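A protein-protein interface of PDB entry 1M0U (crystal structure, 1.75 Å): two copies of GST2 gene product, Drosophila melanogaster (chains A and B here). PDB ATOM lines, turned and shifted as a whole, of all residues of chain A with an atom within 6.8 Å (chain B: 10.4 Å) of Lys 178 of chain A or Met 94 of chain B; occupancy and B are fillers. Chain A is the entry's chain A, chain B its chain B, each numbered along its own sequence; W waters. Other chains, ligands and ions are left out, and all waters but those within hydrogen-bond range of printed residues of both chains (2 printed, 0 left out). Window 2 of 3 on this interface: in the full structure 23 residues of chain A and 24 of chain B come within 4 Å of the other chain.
The side-chain hydroxyl (OG1) of Thr 140 of chain A lies within hydrogen-bond range of the side-chain amide nitrogen (NE2) of Gln 109 of chain B.
The backbone carbonyl oxygen of Ile 136 of chain A lies within hydrogen-bond range of the side-chain hydroxyl of Thr 140 of chain A, 3.0 Å away. The backbone carbonyl oxygen of Lys 178 of chain A lies within hydrogen-bond range of the side-chain hydroxyl of Thr 182 of chain A (3.1 Å).
Ile 136 of chain A touches Val 107 of chain B (CD1 to CB, 3.5 Å). O of His 108 of chain B touches CG1 of Ile 136 of chain A, 3.2 Å away. Ile 136 of chain A touches Gln 109 of chain B. OG1 of Thr 140 of chain A touches CE1 of His 108 of chain B (3.6 Å). CZ of Phe 174 of chain A touches O of Met 94 of chain B (3.2 Å). Lys 178 of chain A touches Met 94 of chain B (NZ to CA, 3.97 Å).
Printed residues of chain B within 4 Å of Thr 140 of chain A: His 108 (3.6 Å) and Gln 109 (3.4 Å). Of chain B, only Met 94 (3.2 Å) comes within 4 Å of Phe 174 of chain A. No residue of chain B comes within 4 Å of Tyr 175 of chain A. Of chain B, only Met 94 (3.97 Å) comes within 4 Å of Lys 178 of chain A. No residue of chain B comes within 4 Å of Leu 179 of chain A. No residue of chain B comes within 4 Å of Thr 182 of chain A. Of chain A, only Phe 174 and Lys 178 come within 4 Å of Met 94 of chain B. Of the printed residues of chain A, Val 107 of chain B touches Ile 136. Of the printed residues of chain A, His 108 of chain B touches Ile 136 (3.2 Å) and Thr 140 (3.6 Å). Of the printed residues of chain A, Gln 109 of chain B touches Ile 136 and Thr 140. The nearest residue of chain A that does not touch Met 94 of chain B is Tyr 175 of chain A (4.03 Å). The nearest printed residue of chain A that does not touch Val 107 of chain B is Thr 140 of chain A (9.1 Å).
Of the 18 printed residues of chain B, 4 touch a printed residue of chain A. Hydrophobic or aromatic side chains of chain B that line the printed part of chain A: Met 94, Val 107 and His 108. Along chain B the printed residues that touch a printed residue of chain A span positions 94 to 109. Hydrophobic or aromatic side chains of chain A that line the printed part of chain B: Ile 136 and Phe 174. Among the printed residues, 7 pairs touch across the chains. Among the printed residues, no Asp or Glu carboxylate lies within 4 Å of a Lys or Arg side-chain nitrogen of the other chain.
No position is printed for both chains.
Water W2 lies within hydrogen-bond range of the side-chain hydroxyl of Thr 140 of chain A and a ring nitrogen (NE2) of His 108 of chain B. Water W1 lies within hydrogen-bond range of OH of Tyr 175 of chain A (2.6 Å) and NE2 of Gln 96 of chain B (3.3 Å).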
ATOM      1  N   ILE A 136     -20.047 -14.033   7.431  1.00  0.00           N
ATOM      2  CA  ILE A 136     -20.880 -12.848   7.178  1.00  0.00           C
ATOM      3  C   ILE A 136     -20.204 -11.597   7.714  1.00  0.00           C
ATOM      4  O   ILE A 136     -20.211 -10.558   7.040  1.00  0.00           O
ATOM      5  CB  ILE A 136     -22.275 -13.012   7.806  1.00  0.00           C
ATOM      6  CG1 ILE A 136     -23.111 -14.012   7.011  1.00  0.00           C
ATOM      7  CG2 ILE A 136     -23.032 -11.645   7.925  1.00  0.00           C
ATOM      8  CD1 ILE A 136     -24.344 -14.453   7.805  1.00  0.00           C
ATOM      9  N   THR A 140     -18.771  -8.385   5.600  1.00  0.00           N
ATOM     10  CA  THR A 140     -19.176  -7.013   5.927  1.00  0.00           C
ATOM     11  C   THR A 140     -17.971  -6.092   6.075  1.00  0.00           C
ATOM     12  O   THR A 140     -17.958  -4.970   5.520  1.00  0.00           O
ATOM     13  CB  THR A 140     -20.057  -7.023   7.193  1.00  0.00           C
ATOM     14  OG1 THR A 140     -21.234  -7.781   6.917  1.00  0.00           O
ATOM     15  CG2 THR A 140     -20.597  -5.615   7.486  1.00  0.00           C
ATOM     16  N   ILE A 172     -19.210   5.232   6.971  1.00  0.00           N
ATOM     17  CA  ILE A 172     -18.398   4.816   8.112  1.00  0.00           C
ATOM     18  C   ILE A 172     -19.264   4.530   9.366  1.00  0.00           C
ATOM     19  O   ILE A 172     -19.141   3.459   9.948  1.00  0.00           O
ATOM     20  CB  ILE A 172     -17.215   5.786   8.377  1.00  0.00           C
ATOM     21  CG1 ILE A 172     -16.126   5.622   7.299  1.00  0.00           C
ATOM     22  CG2 ILE A 172     -16.611   5.533   9.744  1.00  0.00           C
ATOM     23  CD1 ILE A 172     -15.083   6.779   7.246  1.00  0.00           C
ATOM     24  N   PRO A 173     -20.139   5.449   9.791  1.00  0.00           N
ATOM     25  CA  PRO A 173     -21.045   5.137  10.910  1.00  0.00           C
ATOM     26  C   PRO A 173     -21.994   3.957  10.650  1.00  0.00           C
ATOM     27  O   PRO A 173     -22.259   3.195  11.583  1.00  0.00           O
ATOM     28  CB  PRO A 173     -21.858   6.435  11.106  1.00  0.00           C
ATOM     29  CG  PRO A 173     -21.084   7.491  10.413  1.00  0.00           C
ATOM     30  CD  PRO A 173     -20.303   6.834   9.305  1.00  0.00           C
ATOM     31  N   PHE A 174     -22.500   3.809   9.429  1.00  0.00           N
ATOM     32  CA  PHE A 174     -23.432   2.720   9.107  1.00  0.00           C
ATOM     33  C   PHE A 174     -22.760   1.381   9.416  1.00  0.00           C
ATOM     34  O   PHE A 174     -23.327   0.546  10.131  1.00  0.00           O
ATOM     35  CB  PHE A 174     -23.877   2.812   7.641  1.00  0.00           C
ATOM     36  CG  PHE A 174     -24.592   1.588   7.130  1.00  0.00           C
ATOM     37  CD1 PHE A 174     -25.908   1.335   7.489  1.00  0.00           C
ATOM     38  CD2 PHE A 174     -23.941   0.699   6.279  1.00  0.00           C
ATOM     39  CE1 PHE A 174     -26.577   0.205   7.004  1.00  0.00           C
ATOM     40  CE2 PHE A 174     -24.607  -0.427   5.785  1.00  0.00           C
ATOM     41  CZ  PHE A 174     -25.925  -0.667   6.154  1.00  0.00           C
ATOM     42  N   TYR A 175     -21.539   1.202   8.929  1.00  0.00           N
ATOM     43  CA  TYR A 175     -20.816  -0.071   9.134  1.00  0.00           C
ATOM     44  C   TYR A 175     -20.313  -0.234  10.559  1.00  0.00           C
ATOM     45  O   TYR A 175     -20.506  -1.281  11.184  1.00  0.00           O
ATOM     46  CB  TYR A 175     -19.645  -0.189   8.157  1.00  0.00           C
ATOM     47  CG  TYR A 175     -20.091  -0.666   6.802  1.00  0.00           C
ATOM     48  CD1 TYR A 175     -20.184  -2.034   6.526  1.00  0.00           C
ATOM     49  CD2 TYR A 175     -20.458   0.244   5.808  1.00  0.00           C
ATOM     50  CE1 TYR A 175     -20.617  -2.489   5.282  1.00  0.00           C
ATOM     51  CE2 TYR A 175     -20.894  -0.198   4.558  1.00  0.00           C
ATOM     52  CZ  TYR A 175     -20.961  -1.572   4.303  1.00  0.00           C
ATOM     53  OH  TYR A 175     -21.392  -2.022   3.088  1.00  0.00           O
ATOM     54  N   LEU A 176     -19.663   0.797  11.084  1.00  0.00           N
ATOM     55  CA  LEU A 176     -19.007   0.631  12.366  1.00  0.00           C
ATOM     56  C   LEU A 176     -19.999   0.631  13.534  1.00  0.00           C
ATOM     57  O   LEU A 176     -19.767  -0.046  14.526  1.00  0.00           O
ATOM     58  CB  LEU A 176     -17.867   1.640  12.554  1.00  0.00           C
ATOM     59  CG  LEU A 176     -16.686   1.478  11.570  1.00  0.00           C
ATOM     60  CD1 LEU A 176     -15.537   2.474  11.853  1.00  0.00           C
ATOM     61  CD2 LEU A 176     -16.138   0.036  11.599  1.00  0.00           C
ATOM     62  N   GLU A 177     -21.104   1.368  13.426  1.00  0.00           N
ATOM     63  CA  GLU A 177     -22.106   1.289  14.488  1.00  0.00           C
ATOM     64  C   GLU A 177     -22.652  -0.133  14.603  1.00  0.00           C
ATOM     65  O   GLU A 177     -22.839  -0.653  15.708  1.00  0.00           O
ATOM     66  CB  GLU A 177     -23.253   2.266  14.258  1.00  0.00           C
ATOM     67  CG  GLU A 177     -22.889   3.688  14.699  1.00  0.00           C
ATOM     68  CD  GLU A 177     -23.917   4.727  14.291  1.00  0.00           C
ATOM     69  OE1 GLU A 177     -25.039   4.346  13.889  1.00  0.00           O
ATOM     70  OE2 GLU A 177     -23.587   5.936  14.374  1.00  0.00           O
ATOM     71  N   LYS A 178     -22.892  -0.741  13.451  1.00  0.00           N
ATOM     72  CA  LYS A 178     -23.408  -2.112  13.415  1.00  0.00           C
ATOM     73  C   LYS A 178     -22.389  -3.105  13.985  1.00  0.00           C
ATOM     74  O   LYS A 178     -22.746  -3.950  14.808  1.00  0.00           O
ATOM     75  CB  LYS A 178     -23.831  -2.490  12.001  1.00  0.00           C
ATOM     76  CG  LYS A 178     -25.121  -1.801  11.527  1.00  0.00           C
ATOM     77  CD  LYS A 178     -26.391  -2.546  11.915  1.00  0.00           C
ATOM     78  CE  LYS A 178     -27.659  -1.705  11.647  1.00  0.00           C
ATOM     79  NZ  LYS A 178     -27.759  -1.227  10.235  1.00  0.00           N
ATOM     80  N   LEU A 179     -21.123  -2.989  13.588  1.00  0.00           N
ATOM     81  CA  LEU A 179     -20.080  -3.869  14.124  1.00  0.00           C
ATOM     82  C   LEU A 179     -19.869  -3.660  15.629  1.00  0.00           C
ATOM     83  O   LEU A 179     -19.694  -4.614  16.376  1.00  0.00           O
ATOM     84  CB  LEU A 179     -18.771  -3.709  13.342  1.00  0.00           C
ATOM     85  CG  LEU A 179     -18.914  -4.118  11.876  1.00  0.00           C
ATOM     86  CD1 LEU A 179     -17.655  -3.790  11.098  1.00  0.00           C
ATOM     87  CD2 LEU A 179     -19.220  -5.637  11.767  1.00  0.00           C
ATOM     88  N   GLU A 180     -19.916  -2.401  16.074  1.00  0.00           N
ATOM     89  CA  GLU A 180     -19.814  -2.080  17.501  1.00  0.00           C
ATOM     90  C   GLU A 180     -20.884  -2.825  18.300  1.00  0.00           C
ATOM     91  O   GLU A 180     -20.578  -3.432  19.335  1.00  0.00           O
ATOM     92  CB  GLU A 180     -19.953  -0.554  17.722  1.00  0.00           C
ATOM     93  CG  GLU A 180     -19.859  -0.083  19.172  1.00  0.00           C
ATOM     94  CD  GLU A 180     -18.457  -0.033  19.748  1.00  0.00           C
ATOM     95  OE1 GLU A 180     -17.493  -0.459  19.091  1.00  0.00           O
ATOM     96  OE2 GLU A 180     -18.303   0.449  20.912  1.00  0.00           O
ATOM     97  N   GLN A 181     -22.124  -2.774  17.822  1.00  0.00           N
ATOM     98  CA  GLN A 181     -23.239  -3.410  18.534  1.00  0.00           C
ATOM     99  C   GLN A 181     -23.054  -4.932  18.524  1.00  0.00           C
ATOM    100  O   GLN A 181     -23.295  -5.604  19.528  1.00  0.00           O
ATOM    101  CB  GLN A 181     -24.597  -3.024  17.949  1.00  0.00           C
ATOM    102  CG  GLN A 181     -25.783  -3.492  18.804  1.00  0.00           C
ATOM    103  CD  GLN A 181     -25.714  -2.970  20.249  1.00  0.00           C
ATOM    104  OE1 GLN A 181     -25.608  -1.760  20.475  1.00  0.00           O
ATOM    105  NE2 GLN A 181     -25.744  -3.879  21.218  1.00  0.00           N
ATOM    106  N   THR A 182     -22.619  -5.449  17.383  1.00  0.00           N
ATOM    107  CA  THR A 182     -22.298  -6.882  17.269  1.00  0.00           C
ATOM    108  C   THR A 182     -21.313  -7.346  18.334  1.00  0.00           C
ATOM    109  O   THR A 182     -21.534  -8.379  18.983  1.00  0.00           O
ATOM    110  CB  THR A 182     -21.761  -7.167  15.872  1.00  0.00           C
ATOM    111  OG1 THR A 182     -22.828  -7.007  14.924  1.00  0.00           O
ATOM    112  CG2 THR A 182     -21.341  -8.627  15.751  1.00  0.00           C
ATOM    113  N   VAL A 183     -20.243  -6.584  18.547  1.00  0.00           N
ATOM    114  CA  VAL A 183     -19.240  -6.943  19.533  1.00  0.00           C
ATOM    115  C   VAL A 183     -19.837  -6.928  20.936  1.00  0.00           C
ATOM    116  O   VAL A 183     -19.553  -7.811  21.748  1.00  0.00           O
ATOM    117  CB  VAL A 183     -18.039  -5.990  19.459  1.00  0.00           C
ATOM    118  CG1 VAL A 183     -17.104  -6.176  20.623  1.00  0.00           C
ATOM    119  CG2 VAL A 183     -17.291  -6.205  18.147  1.00  0.00           C
ATOM    120  N   ASP A 185     -22.983  -7.469  21.610  1.00  0.00           N
ATOM    121  CA  ASP A 185     -23.888  -8.635  21.649  1.00  0.00           C
ATOM    122  C   ASP A 185     -23.156  -9.992  21.704  1.00  0.00           C
ATOM    123  O   ASP A 185     -23.785 -11.025  21.985  1.00  0.00           O
ATOM    124  CB  ASP A 185     -24.848  -8.626  20.452  1.00  0.00           C
ATOM    125  CG  ASP A 185     -25.815  -7.440  20.461  1.00  0.00           C
ATOM    126  OD1 ASP A 185     -25.966  -6.760  21.504  1.00  0.00           O
ATOM    127  OD2 ASP A 185     -26.467  -7.115  19.447  1.00  0.00           O
ATOM    128  N   TYR A 221     -15.666   4.100  18.695  1.00  0.00           N
ATOM    129  CA  TYR A 221     -16.122   2.705  18.781  1.00  0.00           C
ATOM    130  C   TYR A 221     -15.248   1.898  19.748  1.00  0.00           C
ATOM    131  O   TYR A 221     -14.419   1.075  19.327  1.00  0.00           O
ATOM    132  CB  TYR A 221     -16.158   2.088  17.362  1.00  0.00           C
ATOM    133  CG  TYR A 221     -16.959   2.921  16.391  1.00  0.00           C
ATOM    134  CD1 TYR A 221     -18.340   3.083  16.553  1.00  0.00           C
ATOM    135  CD2 TYR A 221     -16.337   3.611  15.354  1.00  0.00           C
ATOM    136  CE1 TYR A 221     -19.078   3.858  15.700  1.00  0.00           C
ATOM    137  CE2 TYR A 221     -17.074   4.413  14.494  1.00  0.00           C
ATOM    138  CZ  TYR A 221     -18.440   4.537  14.665  1.00  0.00           C
ATOM    139  OH  TYR A 221     -19.184   5.320  13.817  1.00  0.00           O
ATOM    140  N   LEU A 224     -15.056  -1.986  19.499  1.00  0.00           N
ATOM    141  CA  LEU A 224     -14.226  -2.396  18.365  1.00  0.00           C
ATOM    142  C   LEU A 224     -12.733  -2.262  18.655  1.00  0.00           C
ATOM    143  O   LEU A 224     -11.966  -3.171  18.347  1.00  0.00           O
ATOM    144  CB  LEU A 224     -14.639  -1.668  17.080  1.00  0.00           C
ATOM    145  CG  LEU A 224     -15.989  -2.043  16.472  1.00  0.00           C
ATOM    146  CD1 LEU A 224     -16.253  -1.144  15.264  1.00  0.00           C
ATOM    147  CD2 LEU A 224     -16.058  -3.542  16.055  1.00  0.00           C
ATOM    148  N   TRP B  85     -41.098  -2.435   0.862  1.00  0.00           N
ATOM    149  CA  TRP B  85     -39.693  -2.478   1.261  1.00  0.00           C
ATOM    150  C   TRP B  85     -39.328  -1.490   2.394  1.00  0.00           C
ATOM    151  O   TRP B  85     -38.672  -1.885   3.364  1.00  0.00           O
ATOM    152  CB  TRP B  85     -38.792  -2.335   0.017  1.00  0.00           C
ATOM    153  CG  TRP B  85     -37.313  -2.214   0.284  1.00  0.00           C
ATOM    154  CD1 TRP B  85     -36.467  -1.280  -0.234  1.00  0.00           C
ATOM    155  CD2 TRP B  85     -36.510  -3.064   1.112  1.00  0.00           C
ATOM    156  NE1 TRP B  85     -35.189  -1.483   0.231  1.00  0.00           N
ATOM    157  CE2 TRP B  85     -35.187  -2.568   1.066  1.00  0.00           C
ATOM    158  CE3 TRP B  85     -36.775  -4.192   1.906  1.00  0.00           C
ATOM    159  CZ2 TRP B  85     -34.137  -3.158   1.772  1.00  0.00           C
ATOM    160  CZ3 TRP B  85     -35.726  -4.778   2.608  1.00  0.00           C
ATOM    161  CH2 TRP B  85     -34.427  -4.261   2.532  1.00  0.00           C
ATOM    162  N   LEU B  88     -40.132  -3.169   5.691  1.00  0.00           N
ATOM    163  CA  LEU B  88     -39.392  -4.389   6.036  1.00  0.00           C
ATOM    164  C   LEU B  88     -37.891  -4.161   6.187  1.00  0.00           C
ATOM    165  O   LEU B  88     -37.210  -4.917   6.885  1.00  0.00           O
ATOM    166  CB  LEU B  88     -39.668  -5.507   5.016  1.00  0.00           C
ATOM    167  CG  LEU B  88     -41.075  -6.116   4.981  1.00  0.00           C
ATOM    168  CD1 LEU B  88     -41.098  -7.293   4.009  1.00  0.00           C
ATOM    169  CD2 LEU B  88     -41.558  -6.554   6.370  1.00  0.00           C
ATOM    170  N   LYS B  89     -37.383  -3.106   5.553  1.00  0.00           N
ATOM    171  CA  LYS B  89     -35.959  -2.755   5.643  1.00  0.00           C
ATOM    172  C   LYS B  89     -35.347  -2.801   7.061  1.00  0.00           C
ATOM    173  O   LYS B  89     -34.295  -3.430   7.238  1.00  0.00           O
ATOM    174  CB  LYS B  89     -35.671  -1.422   4.942  1.00  0.00           C
ATOM    175  CG  LYS B  89     -34.191  -1.070   4.822  1.00  0.00           C
ATOM    176  CD  LYS B  89     -33.985   0.121   3.905  1.00  0.00           C
ATOM    177  CE  LYS B  89     -32.522   0.506   3.845  1.00  0.00           C
ATOM    178  NZ  LYS B  89     -32.242   1.374   2.664  1.00  0.00           N
ATOM    179  N   PRO B  90     -35.971  -2.173   8.073  1.00  0.00           N
ATOM    180  CA  PRO B  90     -35.420  -2.212   9.437  1.00  0.00           C
ATOM    181  C   PRO B  90     -35.335  -3.616  10.063  1.00  0.00           C
ATOM    182  O   PRO B  90     -34.640  -3.781  11.071  1.00  0.00           O
ATOM    183  CB  PRO B  90     -36.402  -1.329  10.234  1.00  0.00           C
ATOM    184  CG  PRO B  90     -37.009  -0.466   9.211  1.00  0.00           C
ATOM    185  CD  PRO B  90     -37.205  -1.367   8.021  1.00  0.00           C
ATOM    186  N   THR B  91     -36.014  -4.607   9.476  1.00  0.00           N
ATOM    187  CA  THR B  91     -36.005  -5.957  10.031  1.00  0.00           C
ATOM    188  C   THR B  91     -34.950  -6.821   9.346  1.00  0.00           C
ATOM    189  O   THR B  91     -34.801  -7.998   9.679  1.00  0.00           O
ATOM    190  CB  THR B  91     -37.381  -6.627   9.907  1.00  0.00           C
ATOM    191  OG1 THR B  91     -37.671  -6.885   8.527  1.00  0.00           O
ATOM    192  CG2 THR B  91     -38.498  -5.674  10.352  1.00  0.00           C
ATOM    193  N   MET B  92     -34.241  -6.234   8.387  1.00  0.00           N
ATOM    194  CA  MET B  92     -33.158  -6.930   7.683  1.00  0.00           C
ATOM    195  C   MET B  92     -31.807  -6.516   8.255  1.00  0.00           C
ATOM    196  O   MET B  92     -31.578  -5.325   8.515  1.00  0.00           O
ATOM    197  CB  MET B  92     -33.217  -6.631   6.178  1.00  0.00           C
ATOM    198  CG  MET B  92     -34.548  -6.949   5.523  1.00  0.00           C
ATOM    199  SD  MET B  92     -34.957  -8.728   5.562  1.00  0.00           S
ATOM    200  CE  MET B  92     -36.637  -8.684   5.185  1.00  0.00           C
ATOM    201  N   PRO B  93     -30.905  -7.474   8.469  1.00  0.00           N
ATOM    202  CA  PRO B  93     -29.541  -7.123   8.871  1.00  0.00           C
ATOM    203  C   PRO B  93     -28.975  -6.146   7.843  1.00  0.00           C
ATOM    204  O   PRO B  93     -29.123  -6.348   6.628  1.00  0.00           O
ATOM    205  CB  PRO B  93     -28.781  -8.458   8.812  1.00  0.00           C
ATOM    206  CG  PRO B  93     -29.816  -9.523   8.850  1.00  0.00           C
ATOM    207  CD  PRO B  93     -31.104  -8.935   8.339  1.00  0.00           C
ATOM    208  N   MET B  94     -28.367  -5.070   8.324  1.00  0.00           N
ATOM    209  CA  MET B  94     -27.774  -4.055   7.442  1.00  0.00           C
ATOM    210  C   MET B  94     -28.741  -3.427   6.438  1.00  0.00           C
ATOM    211  O   MET B  94     -28.299  -2.782   5.486  1.00  0.00           O
ATOM    212  CB  MET B  94     -26.576  -4.614   6.651  1.00  0.00           C
ATOM    213  CG  MET B  94     -25.626  -5.477   7.424  1.00  0.00           C
ATOM    214  SD  MET B  94     -24.478  -4.566   8.438  1.00  0.00           S
ATOM    215  CE  MET B  94     -23.946  -3.269   7.424  1.00  0.00           C
ATOM    216  N   GLY B  95     -30.043  -3.643   6.623  1.00  0.00           N
ATOM    217  CA  GLY B  95     -31.047  -3.082   5.730  1.00  0.00           C
ATOM    218  C   GLY B  95     -30.913  -3.492   4.277  1.00  0.00           C
ATOM    219  O   GLY B  95     -31.302  -2.746   3.378  1.00  0.00           O
ATOM    220  N   GLN B  96     -30.369  -4.680   4.027  1.00  0.00           N
ATOM    221  CA  GLN B  96     -30.269  -5.152   2.648  1.00  0.00           C
ATOM    222  C   GLN B  96     -30.806  -6.567   2.461  1.00  0.00           C
ATOM    223  O   GLN B  96     -31.119  -7.247   3.420  1.00  0.00           O
ATOM    224  CB  GLN B  96     -28.843  -5.051   2.115  1.00  0.00           C
ATOM    225  CG  GLN B  96     -27.739  -5.512   3.061  1.00  0.00           C
ATOM    226  CD  GLN B  96     -26.368  -4.960   2.668  1.00  0.00           C
ATOM    227  OE1 GLN B  96     -26.269  -4.072   1.819  1.00  0.00           O
ATOM    228  NE2 GLN B  96     -25.317  -5.481   3.282  1.00  0.00           N
ATOM    229  N   MET B  97     -30.934  -6.960   1.201  1.00  0.00           N
ATOM    230  CA  MET B  97     -31.355  -8.303   0.809  1.00  0.00           C
ATOM    231  C   MET B  97     -30.397  -8.737  -0.305  1.00  0.00           C
ATOM    232  O   MET B  97     -29.730  -7.889  -0.896  1.00  0.00           O
ATOM    233  CB  MET B  97     -32.820  -8.286   0.337  1.00  0.00           C
ATOM    234  CG  MET B  97     -33.836  -7.954   1.460  1.00  0.00           C
ATOM    235  SD  MET B  97     -35.556  -8.102   1.001  1.00  0.00           S
ATOM    236  CE  MET B  97     -35.677  -7.000  -0.342  1.00  0.00           C
ATOM    237  N   PRO B  98     -30.296 -10.030  -0.613  1.00  0.00           N
ATOM    238  CA  PRO B  98     -31.090 -11.110  -0.002  1.00  0.00           C
ATOM    239  C   PRO B  98     -30.819 -11.347   1.480  1.00  0.00           C
ATOM    240  O   PRO B  98     -29.729 -11.081   1.984  1.00  0.00           O
ATOM    241  CB  PRO B  98     -30.658 -12.364  -0.780  1.00  0.00           C
ATOM    242  CG  PRO B  98     -29.815 -11.908  -1.891  1.00  0.00           C
ATOM    243  CD  PRO B  98     -29.373 -10.506  -1.658  1.00  0.00           C
ATOM    244  N   VAL B  99     -31.847 -11.855   2.167  1.00  0.00           N
ATOM    245  CA  VAL B  99     -31.727 -12.352   3.523  1.00  0.00           C
ATOM    246  C   VAL B  99     -32.347 -13.748   3.599  1.00  0.00           C
ATOM    247  O   VAL B  99     -33.352 -14.019   2.945  1.00  0.00           O
ATOM    248  CB  VAL B  99     -32.437 -11.381   4.526  1.00  0.00           C
ATOM    249  CG1 VAL B  99     -32.772 -12.047   5.817  1.00  0.00           C
ATOM    250  CG2 VAL B  99     -31.554 -10.139   4.785  1.00  0.00           C
ATOM    251  N   ARG B 106     -31.941 -14.482  11.245  1.00  0.00           N
ATOM    252  CA  ARG B 106     -31.712 -13.891   9.930  1.00  0.00           C
ATOM    253  C   ARG B 106     -30.250 -13.706   9.625  1.00  0.00           C
ATOM    254  O   ARG B 106     -29.466 -13.260  10.476  1.00  0.00           O
ATOM    255  CB  ARG B 106     -32.449 -12.563   9.770  1.00  0.00           C
ATOM    256  CG  ARG B 106     -33.954 -12.721   9.778  1.00  0.00           C
ATOM    257  CD  ARG B 106     -34.746 -11.443   9.612  1.00  0.00           C
ATOM    258  NE  ARG B 106     -36.150 -11.792   9.404  1.00  0.00           N
ATOM    259  CZ  ARG B 106     -37.072 -11.004   8.881  1.00  0.00           C
ATOM    260  NH1 ARG B 106     -36.782  -9.763   8.505  1.00  0.00           N
ATOM    261  NH2 ARG B 106     -38.305 -11.466   8.746  1.00  0.00           N
ATOM    262  N   VAL B 107     -29.894 -14.020   8.387  1.00  0.00           N
ATOM    263  CA  VAL B 107     -28.532 -13.837   7.925  1.00  0.00           C
ATOM    264  C   VAL B 107     -28.567 -13.079   6.605  1.00  0.00           C
ATOM    265  O   VAL B 107     -29.610 -12.968   5.982  1.00  0.00           O
ATOM    266  CB  VAL B 107     -27.791 -15.205   7.771  1.00  0.00           C
ATOM    267  CG1 VAL B 107     -27.360 -15.725   9.140  1.00  0.00           C
ATOM    268  CG2 VAL B 107     -28.671 -16.226   7.035  1.00  0.00           C
ATOM    269  N   HIS B 108     -27.423 -12.524   6.197  1.00  0.00           N
ATOM    270  CA  HIS B 108     -27.331 -11.832   4.919  1.00  0.00           C
ATOM    271  C   HIS B 108     -25.965 -12.181   4.311  1.00  0.00           C
ATOM    272  O   HIS B 108     -25.245 -13.025   4.866  1.00  0.00           O
ATOM    273  CB  HIS B 108     -27.518 -10.298   5.087  1.00  0.00           C
ATOM    274  CG  HIS B 108     -26.448  -9.650   5.911  1.00  0.00           C
ATOM    275  ND1 HIS B 108     -25.644  -8.646   5.422  1.00  0.00           N
ATOM    276  CD2 HIS B 108     -26.058  -9.858   7.190  1.00  0.00           C
ATOM    277  CE1 HIS B 108     -24.778  -8.290   6.353  1.00  0.00           C
ATOM    278  NE2 HIS B 108     -25.018  -8.997   7.440  1.00  0.00           N
ATOM    279  N   GLN B 109     -25.629 -11.530   3.197  1.00  0.00           N
ATOM    280  CA  GLN B 109     -24.384 -11.731   2.435  1.00  0.00           C
ATOM    281  C   GLN B 109     -24.554 -12.960   1.543  1.00  0.00           C
ATOM    282  O   GLN B 109     -24.317 -14.092   1.977  1.00  0.00           O
ATOM    283  CB  GLN B 109     -23.130 -11.837   3.322  1.00  0.00           C
ATOM    284  CG  GLN B 109     -22.736 -10.517   4.002  1.00  0.00           C
ATOM    285  CD  GLN B 109     -22.100  -9.510   3.046  1.00  0.00           C
ATOM    286  OE1 GLN B 109     -21.982  -9.763   1.838  1.00  0.00           O
ATOM    287  NE2 GLN B 109     -21.640  -8.380   3.595  1.00  0.00           N
ATOM    288  N   SER B 110     -24.998 -12.720   0.311  1.00  0.00           N
ATOM    289  CA  SER B 110     -25.454 -13.796  -0.569  1.00  0.00           C
ATOM    290  C   SER B 110     -24.397 -14.852  -0.902  1.00  0.00           C
ATOM    291  O   SER B 110     -24.740 -16.022  -1.065  1.00  0.00           O
ATOM    292  CB  SER B 110     -26.072 -13.234  -1.852  1.00  0.00           C
ATOM    293  OG  SER B 110     -25.089 -12.524  -2.583  1.00  0.00           O
HETATM  294  O   HOH W   1     -22.140  -4.539   3.169  1.00  0.00           O
HETATM  295  O   HOH W   2     -22.713  -8.080   8.996  1.00  0.00           O
